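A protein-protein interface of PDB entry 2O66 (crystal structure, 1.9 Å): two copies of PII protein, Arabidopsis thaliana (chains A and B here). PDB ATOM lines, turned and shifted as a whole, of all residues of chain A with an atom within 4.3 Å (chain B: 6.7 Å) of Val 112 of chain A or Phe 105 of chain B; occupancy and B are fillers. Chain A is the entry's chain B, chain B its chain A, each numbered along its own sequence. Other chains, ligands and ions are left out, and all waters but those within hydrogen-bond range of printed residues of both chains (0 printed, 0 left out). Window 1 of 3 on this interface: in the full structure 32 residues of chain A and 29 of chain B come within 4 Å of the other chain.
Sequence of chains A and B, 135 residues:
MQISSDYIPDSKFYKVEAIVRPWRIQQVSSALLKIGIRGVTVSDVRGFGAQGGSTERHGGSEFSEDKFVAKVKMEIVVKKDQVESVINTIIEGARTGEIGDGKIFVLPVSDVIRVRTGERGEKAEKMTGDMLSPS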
ATOM      1  N   PHE A  13     -21.724  16.721  -1.058  1.00  0.00           N
ATOM      2  CA  PHE A  13     -22.686  15.905  -1.799  1.00  0.00           C
ATOM      3  C   PHE A  13     -24.036  16.596  -1.865  1.00  0.00           C
ATOM      4  O   PHE A  13     -24.371  17.402  -0.994  1.00  0.00           O
ATOM      5  CB  PHE A  13     -22.863  14.535  -1.134  1.00  0.00           C
ATOM      6  CG  PHE A  13     -21.622  13.690  -1.145  1.00  0.00           C
ATOM      7  CD1 PHE A  13     -21.294  12.927  -2.262  1.00  0.00           C
ATOM      8  CD2 PHE A  13     -20.778  13.659  -0.038  1.00  0.00           C
ATOM      9  CE1 PHE A  13     -20.141  12.144  -2.281  1.00  0.00           C
ATOM     10  CE2 PHE A  13     -19.624  12.881  -0.046  1.00  0.00           C
ATOM     11  CZ  PHE A  13     -19.304  12.120  -1.174  1.00  0.00           C
ATOM     12  N   VAL A  77     -27.910  10.697  -5.396  1.00  0.00           N
ATOM     13  CA  VAL A  77     -26.981  11.450  -4.573  1.00  0.00           C
ATOM     14  C   VAL A  77     -25.619  11.449  -5.258  1.00  0.00           C
ATOM     15  O   VAL A  77     -25.063  10.390  -5.560  1.00  0.00           O
ATOM     16  CB  VAL A  77     -26.915  10.899  -3.122  1.00  0.00           C
ATOM     17  CG1 VAL A  77     -25.833  11.608  -2.320  1.00  0.00           C
ATOM     18  CG2 VAL A  77     -28.273  11.066  -2.438  1.00  0.00           C
ATOM     19  N   VAL A 109     -26.510  17.084   0.995  1.00  0.00           N
ATOM     20  CA  VAL A 109     -26.318  15.821   1.707  1.00  0.00           C
ATOM     21  C   VAL A 109     -24.984  15.888   2.462  1.00  0.00           C
ATOM     22  O   VAL A 109     -23.926  16.054   1.851  1.00  0.00           O
ATOM     23  CB  VAL A 109     -26.350  14.598   0.738  1.00  0.00           C
ATOM     24  CG1 VAL A 109     -25.870  13.331   1.436  1.00  0.00           C
ATOM     25  CG2 VAL A 109     -27.757  14.386   0.183  1.00  0.00           C
ATOM     26  N   ASP A 111     -23.568  13.522   4.432  1.00  0.00           N
ATOM     27  CA  ASP A 111     -22.829  12.256   4.467  1.00  0.00           C
ATOM     28  C   ASP A 111     -23.467  11.173   3.614  1.00  0.00           C
ATOM     29  O   ASP A 111     -24.685  11.090   3.520  1.00  0.00           O
ATOM     30  CB  ASP A 111     -22.748  11.736   5.902  1.00  0.00           C
ATOM     31  CG  ASP A 111     -21.383  11.918   6.512  1.00  0.00           C
ATOM     32  OD1 ASP A 111     -20.402  11.386   5.943  1.00  0.00           O
ATOM     33  OD2 ASP A 111     -21.302  12.572   7.573  1.00  0.00           O
ATOM     34  N   VAL A 112     -22.629  10.335   3.007  1.00  0.00           N
ATOM     35  CA  VAL A 112     -23.086   9.117   2.334  1.00  0.00           C
ATOM     36  C   VAL A 112     -22.322   7.945   2.937  1.00  0.00           C
ATOM     37  O   VAL A 112     -21.096   8.003   3.059  1.00  0.00           O
ATOM     38  CB  VAL A 112     -22.851   9.160   0.804  1.00  0.00           C
ATOM     39  CG1 VAL A 112     -23.460   7.925   0.126  1.00  0.00           C
ATOM     40  CG2 VAL A 112     -23.435  10.424   0.203  1.00  0.00           C
ATOM     41  N   ILE A 113     -23.048   6.898   3.328  1.00  0.00           N
ATOM     42  CA  ILE A 113     -22.446   5.712   3.936  1.00  0.00           C
ATOM     43  C   ILE A 113     -22.899   4.450   3.203  1.00  0.00           C
ATOM     44  O   ILE A 113     -24.089   4.280   2.931  1.00  0.00           O
ATOM     45  CB  ILE A 113     -22.800   5.591   5.457  1.00  0.00           C
ATOM     46  CG1 ILE A 113     -22.406   6.857   6.227  1.00  0.00           C
ATOM     47  CG2 ILE A 113     -22.122   4.384   6.083  1.00  0.00           C
ATOM     48  CD1 ILE A 113     -23.555   7.837   6.451  1.00  0.00           C
ATOM     49  N   GLU A 119     -18.050   2.223   4.575  1.00  0.00           N
ATOM     50  CA  GLU A 119     -17.350   3.254   3.807  1.00  0.00           C
ATOM     51  C   GLU A 119     -18.172   4.531   3.784  1.00  0.00           C
ATOM     52  O   GLU A 119     -19.400   4.488   3.725  1.00  0.00           O
ATOM     53  CB  GLU A 119     -17.075   2.802   2.378  1.00  0.00           C
ATOM     54  CG  GLU A 119     -15.916   1.832   2.241  1.00  0.00           C
ATOM     55  CD  GLU A 119     -15.862   1.200   0.864  1.00  0.00           C
ATOM     56  OE1 GLU A 119     -16.866   0.580   0.444  1.00  0.00           O
ATOM     57  OE2 GLU A 119     -14.812   1.325   0.203  1.00  0.00           O
ATOM     58  N   ARG A 120     -17.479   5.661   3.818  1.00  0.00           N
ATOM     59  CA  ARG A 120     -18.113   6.947   4.018  1.00  0.00           C
ATOM     60  C   ARG A 120     -17.508   7.984   3.080  1.00  0.00           C
ATOM     61  O   ARG A 120     -16.290   8.030   2.912  1.00  0.00           O
ATOM     62  CB  ARG A 120     -17.908   7.358   5.472  1.00  0.00           C
ATOM     63  CG  ARG A 120     -18.905   8.335   6.010  1.00  0.00           C
ATOM     64  CD  ARG A 120     -18.951   8.197   7.521  1.00  0.00           C
ATOM     65  NE  ARG A 120     -19.697   9.279   8.147  1.00  0.00           N
ATOM     66  CZ  ARG A 120     -20.142   9.259   9.399  1.00  0.00           C
ATOM     67  NH1 ARG A 120     -19.927   8.204  10.177  1.00  0.00           N
ATOM     68  NH2 ARG A 120     -20.810  10.297   9.868  1.00  0.00           N
ATOM     69  N   GLY A 121     -18.358   8.808   2.470  1.00  0.00           N
ATOM     70  CA  GLY A 121     -17.899   9.854   1.558  1.00  0.00           C
ATOM     71  C   GLY A 121     -17.743   9.388   0.122  1.00  0.00           C
ATOM     72  O   GLY A 121     -18.611   8.696  -0.409  1.00  0.00           O
ATOM     73  N   ALA A 124     -18.150   5.877  -0.884  1.00  0.00           N
ATOM     74  CA  ALA A 124     -19.495   5.359  -0.622  1.00  0.00           C
ATOM     75  C   ALA A 124     -20.556   5.795  -1.634  1.00  0.00           C
ATOM     76  O   ALA A 124     -21.656   5.243  -1.652  1.00  0.00           O
ATOM     77  CB  ALA A 124     -19.933   5.741   0.789  1.00  0.00           C
ATOM     78  N   GLU A 125     -20.239   6.779  -2.469  1.00  0.00           N
ATOM     79  CA  GLU A 125     -21.262   7.377  -3.326  1.00  0.00           C
ATOM     80  C   GLU A 125     -21.629   6.554  -4.569  1.00  0.00           C
ATOM     81  O   GLU A 125     -22.788   6.538  -4.976  1.00  0.00           O
ATOM     82  CB  GLU A 125     -20.915   8.838  -3.669  1.00  0.00           C
ATOM     83  CG  GLU A 125     -19.897   9.051  -4.780  1.00  0.00           C
ATOM     84  CD  GLU A 125     -20.537   9.538  -6.072  1.00  0.00           C
ATOM     85  OE1 GLU A 125     -21.367   8.803  -6.648  1.00  0.00           O
ATOM     86  OE2 GLU A 125     -20.206  10.659  -6.516  1.00  0.00           O
ATOM     87  N   LYS B  15     -31.830  14.561   8.948  1.00  0.00           N
ATOM     88  CA  LYS B  15     -32.567  13.382   8.526  1.00  0.00           C
ATOM     89  C   LYS B  15     -31.562  12.304   8.170  1.00  0.00           C
ATOM     90  O   LYS B  15     -30.628  12.542   7.396  1.00  0.00           O
ATOM     91  CB  LYS B  15     -33.457  13.675   7.318  1.00  0.00           C
ATOM     92  CG  LYS B  15     -34.114  12.413   6.750  1.00  0.00           C
ATOM     93  CD  LYS B  15     -34.771  12.649   5.408  1.00  0.00           C
ATOM     94  CE  LYS B  15     -36.162  13.218   5.576  1.00  0.00           C
ATOM     95  NZ  LYS B  15     -36.831  13.328   4.253  1.00  0.00           N
ATOM     96  N   VAL B  16     -31.747  11.128   8.753  1.00  0.00           N
ATOM     97  CA  VAL B  16     -30.974   9.952   8.379  1.00  0.00           C
ATOM     98  C   VAL B  16     -31.897   9.096   7.528  1.00  0.00           C
ATOM     99  O   VAL B  16     -32.970   8.671   7.976  1.00  0.00           O
ATOM    100  CB  VAL B  16     -30.454   9.171   9.605  1.00  0.00           C
ATOM    101  CG1 VAL B  16     -29.583   7.990   9.165  1.00  0.00           C
ATOM    102  CG2 VAL B  16     -29.654  10.090  10.512  1.00  0.00           C
ATOM    103  N   GLU B  17     -31.472   8.881   6.290  1.00  0.00           N
ATOM    104  CA  GLU B  17     -32.274   8.240   5.266  1.00  0.00           C
ATOM    105  C   GLU B  17     -31.547   6.975   4.828  1.00  0.00           C
ATOM    106  O   GLU B  17     -30.473   7.057   4.233  1.00  0.00           O
ATOM    107  CB  GLU B  17     -32.384   9.213   4.095  1.00  0.00           C
ATOM    108  CG  GLU B  17     -33.481   8.963   3.112  1.00  0.00           C
ATOM    109  CD  GLU B  17     -33.629  10.135   2.162  1.00  0.00           C
ATOM    110  OE1 GLU B  17     -32.816  10.248   1.223  1.00  0.00           O
ATOM    111  OE2 GLU B  17     -34.550  10.956   2.361  1.00  0.00           O
ATOM    112  N   ALA B  18     -32.113   5.811   5.142  1.00  0.00           N
ATOM    113  CA  ALA B  18     -31.467   4.537   4.835  1.00  0.00           C
ATOM    114  C   ALA B  18     -32.250   3.756   3.780  1.00  0.00           C
ATOM    115  O   ALA B  18     -33.430   3.470   3.964  1.00  0.00           O
ATOM    116  CB  ALA B  18     -31.314   3.707   6.096  1.00  0.00           C
ATOM    117  N   ILE B  19     -31.585   3.413   2.682  1.00  0.00           N
ATOM    118  CA  ILE B  19     -32.207   2.605   1.635  1.00  0.00           C
ATOM    119  C   ILE B  19     -31.642   1.208   1.786  1.00  0.00           C
ATOM    120  O   ILE B  19     -30.480   0.984   1.468  1.00  0.00           O
ATOM    121  CB  ILE B  19     -31.875   3.131   0.212  1.00  0.00           C
ATOM    122  CG1 ILE B  19     -32.011   4.655   0.126  1.00  0.00           C
ATOM    123  CG2 ILE B  19     -32.729   2.421  -0.849  1.00  0.00           C
ATOM    124  CD1 ILE B  19     -33.404   5.177   0.309  1.00  0.00           C
ATOM    125  N   LYS B 103     -27.578   2.010   1.081  1.00  0.00           N
ATOM    126  CA  LYS B 103     -26.806   3.188   1.483  1.00  0.00           C
ATOM    127  C   LYS B 103     -27.550   3.993   2.541  1.00  0.00           C
ATOM    128  O   LYS B 103     -28.771   3.882   2.670  1.00  0.00           O
ATOM    129  CB  LYS B 103     -26.545   4.101   0.278  1.00  0.00           C
ATOM    130  CG  LYS B 103     -25.641   3.529  -0.803  1.00  0.00           C
ATOM    131  CD  LYS B 103     -25.385   4.565  -1.897  1.00  0.00           C
ATOM    132  CE  LYS B 103     -24.682   3.962  -3.108  1.00  0.00           C
ATOM    133  NZ  LYS B 103     -23.295   3.519  -2.801  1.00  0.00           N
ATOM    134  N   ILE B 104     -26.808   4.813   3.279  1.00  0.00           N
ATOM    135  CA  ILE B 104     -27.401   5.770   4.219  1.00  0.00           C
ATOM    136  C   ILE B 104     -27.023   7.180   3.785  1.00  0.00           C
ATOM    137  O   ILE B 104     -25.859   7.449   3.485  1.00  0.00           O
ATOM    138  CB  ILE B 104     -26.905   5.532   5.669  1.00  0.00           C
ATOM    139  CG1 ILE B 104     -27.334   4.146   6.163  1.00  0.00           C
ATOM    140  CG2 ILE B 104     -27.408   6.641   6.602  1.00  0.00           C
ATOM    141  CD1 ILE B 104     -26.482   3.604   7.305  1.00  0.00           C
ATOM    142  N   PHE B 105     -28.013   8.067   3.727  1.00  0.00           N
ATOM    143  CA  PHE B 105     -27.757   9.472   3.449  1.00  0.00           C
ATOM    144  C   PHE B 105     -28.106  10.303   4.670  1.00  0.00           C
ATOM    145  O   PHE B 105     -29.028   9.967   5.420  1.00  0.00           O
ATOM    146  CB  PHE B 105     -28.550   9.951   2.230  1.00  0.00           C
ATOM    147  CG  PHE B 105     -28.394   9.070   1.018  1.00  0.00           C
ATOM    148  CD1 PHE B 105     -27.154   8.912   0.407  1.00  0.00           C
ATOM    149  CD2 PHE B 105     -29.495   8.407   0.484  1.00  0.00           C
ATOM    150  CE1 PHE B 105     -27.008   8.091  -0.716  1.00  0.00           C
ATOM    151  CE2 PHE B 105     -29.361   7.588  -0.638  1.00  0.00           C
ATOM    152  CZ  PHE B 105     -28.113   7.431  -1.240  1.00  0.00           C
ATOM    153  N   VAL B 106     -27.354  11.381   4.870  1.00  0.00           N
ATOM    154  CA  VAL B 106     -27.600  12.299   5.974  1.00  0.00           C
ATOM    155  C   VAL B 106     -27.803  13.691   5.395  1.00  0.00           C
ATOM    156  O   VAL B 106     -26.949  14.194   4.662  1.00  0.00           O
ATOM    157  CB  VAL B 106     -26.438  12.308   6.991  1.00  0.00           C
ATOM    158  CG1 VAL B 106     -26.783  13.203   8.187  1.00  0.00           C
ATOM    159  CG2 VAL B 106     -26.114  10.889   7.461  1.00  0.00           C
ATOM    160  N   LEU B 107     -28.945  14.294   5.713  1.00  0.00           N
ATOM    161  CA  LEU B 107     -29.311  15.609   5.187  1.00  0.00           C
ATOM    162  C   LEU B 107     -29.682  16.547   6.329  1.00  0.00           C
ATOM    163  O   LEU B 107     -30.388  16.131   7.256  1.00  0.00           O
ATOM    164  CB  LEU B 107     -30.501  15.504   4.225  1.00  0.00           C
ATOM    165  CG  LEU B 107     -30.420  14.539   3.035  1.00  0.00           C
ATOM    166  CD1 LEU B 107     -31.044  13.188   3.392  1.00  0.00           C
ATOM    167  CD2 LEU B 107     -31.120  15.143   1.830  1.00  0.00           C
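N of Lys 15 of chain B is in hydrogen-bond range of O of Leu 107 of chain B (2.7 Å).
O of Glu 17 of chain B is in hydrogen-bond range of N of Phe 105 of chain B (2.7 Å).
The backbone NH of Ile 19 of chain B lies within hydrogen-bond range of the backbone carbonyl oxygen of Lys 103 of chain B.
O of Phe 13 of chain A sits at hydrogen-bond distance from N of Val 109 of chain A.
OD1 of Asp 111 of chain A lies within salt-bridge range of NE of Arg 120 of chain A (3.1 Å).
The backbone NH of Gly 121 of chain A is in hydrogen-bond range of the backbone carbonyl oxygen of Val 112 of chain A (2.9 Å).
Val 77 of chain A touches Phe 105 of chain B (CG2 to CE1, 3.7 Å).
Val 109 of chain A touches Val 106 of chain B.
Leu 107 of chain B touches Val 109 of chain A (CD2 to CG2, 3.8 Å).
Asp 111 of chain A touches Ile 104 of chain B.
Asp 111 of chain A touches Phe 105 of chain B.
Ile 104 of chain B touches Val 112 of chain A (O to CA, 3.4 Å).
CE1 of Phe 105 of chain B touches CG1 of Val 112 of chain A, 3.7 Å away.
Ile 113 of chain A touches Lys 103 of chain B.
Lys 103 of chain B touches Glu 125 of chain A (CE to O, 3.7 Å).
Printed residues of chain B within 4 Å of Asp 111 of chain A: Ile 104 (3.8 Å), Phe 105 (3.5 Å) and Val 106 (3.0 Å).
Printed residues of chain B within 4 Å of Val 112 of chain A: Ile 104 and Phe 105.
Printed residues of chain A within 4 Å of Lys 103 of chain B: Ile 113, Ala 124 and Glu 125.
Of the printed residues of chain A, Phe 105 of chain B touches Val 77 (3.7 Å), Asp 111 (3.5 Å) and Val 112 (3.7 Å).
The nearest residue of chain B that does not touch Val 112 of chain A is Lys 103 of chain B (4.4 Å).
The nearest printed residue of chain A that does not touch Phe 105 of chain B is Val 109 of chain A (4.4 Å).
The nearest printed residue of chain B that does not touch Val 109 of chain A is Phe 105 of chain B (4.4 Å).
No position is printed for both chains.
Of the 12 pairs that touch across the chains among the printed residues, none has its exchanged pair printed and touching as well.
Of the 10 printed residues of chain B, 5 touch a printed residue of chain A.
Hydrophobic or aromatic side chains of chain B within 4 Å of the printed part of chain A: Phe 105, Val 106 and Leu 107.
Printed residues of chain A that touch a printed residue of chain B: Val 77, Val 109, Asp 111, Val 112, Ile 113, Ala 124 and Glu 125.
Hydrophobic or aromatic side chains of chain A that line the printed part of chain B: Val 77, Val 109, Val 112 and Ile 113.
The backbone carbonyl oxygen (O) of Ala 124 of chain A sits at hydrogen-bond distance from the side-chain amino group (NZ) of Lys 103 of chain B (2.6 Å).
The backbone carbonyl oxygen of Ile 113 of chain A sits at hydrogen-bond distance from the backbone NH of Ile 104 of chain B (2.8 Å).
O of Asp 111 of chain A is in hydrogen-bond range of N of Val 106 of chain B (3.0 Å).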
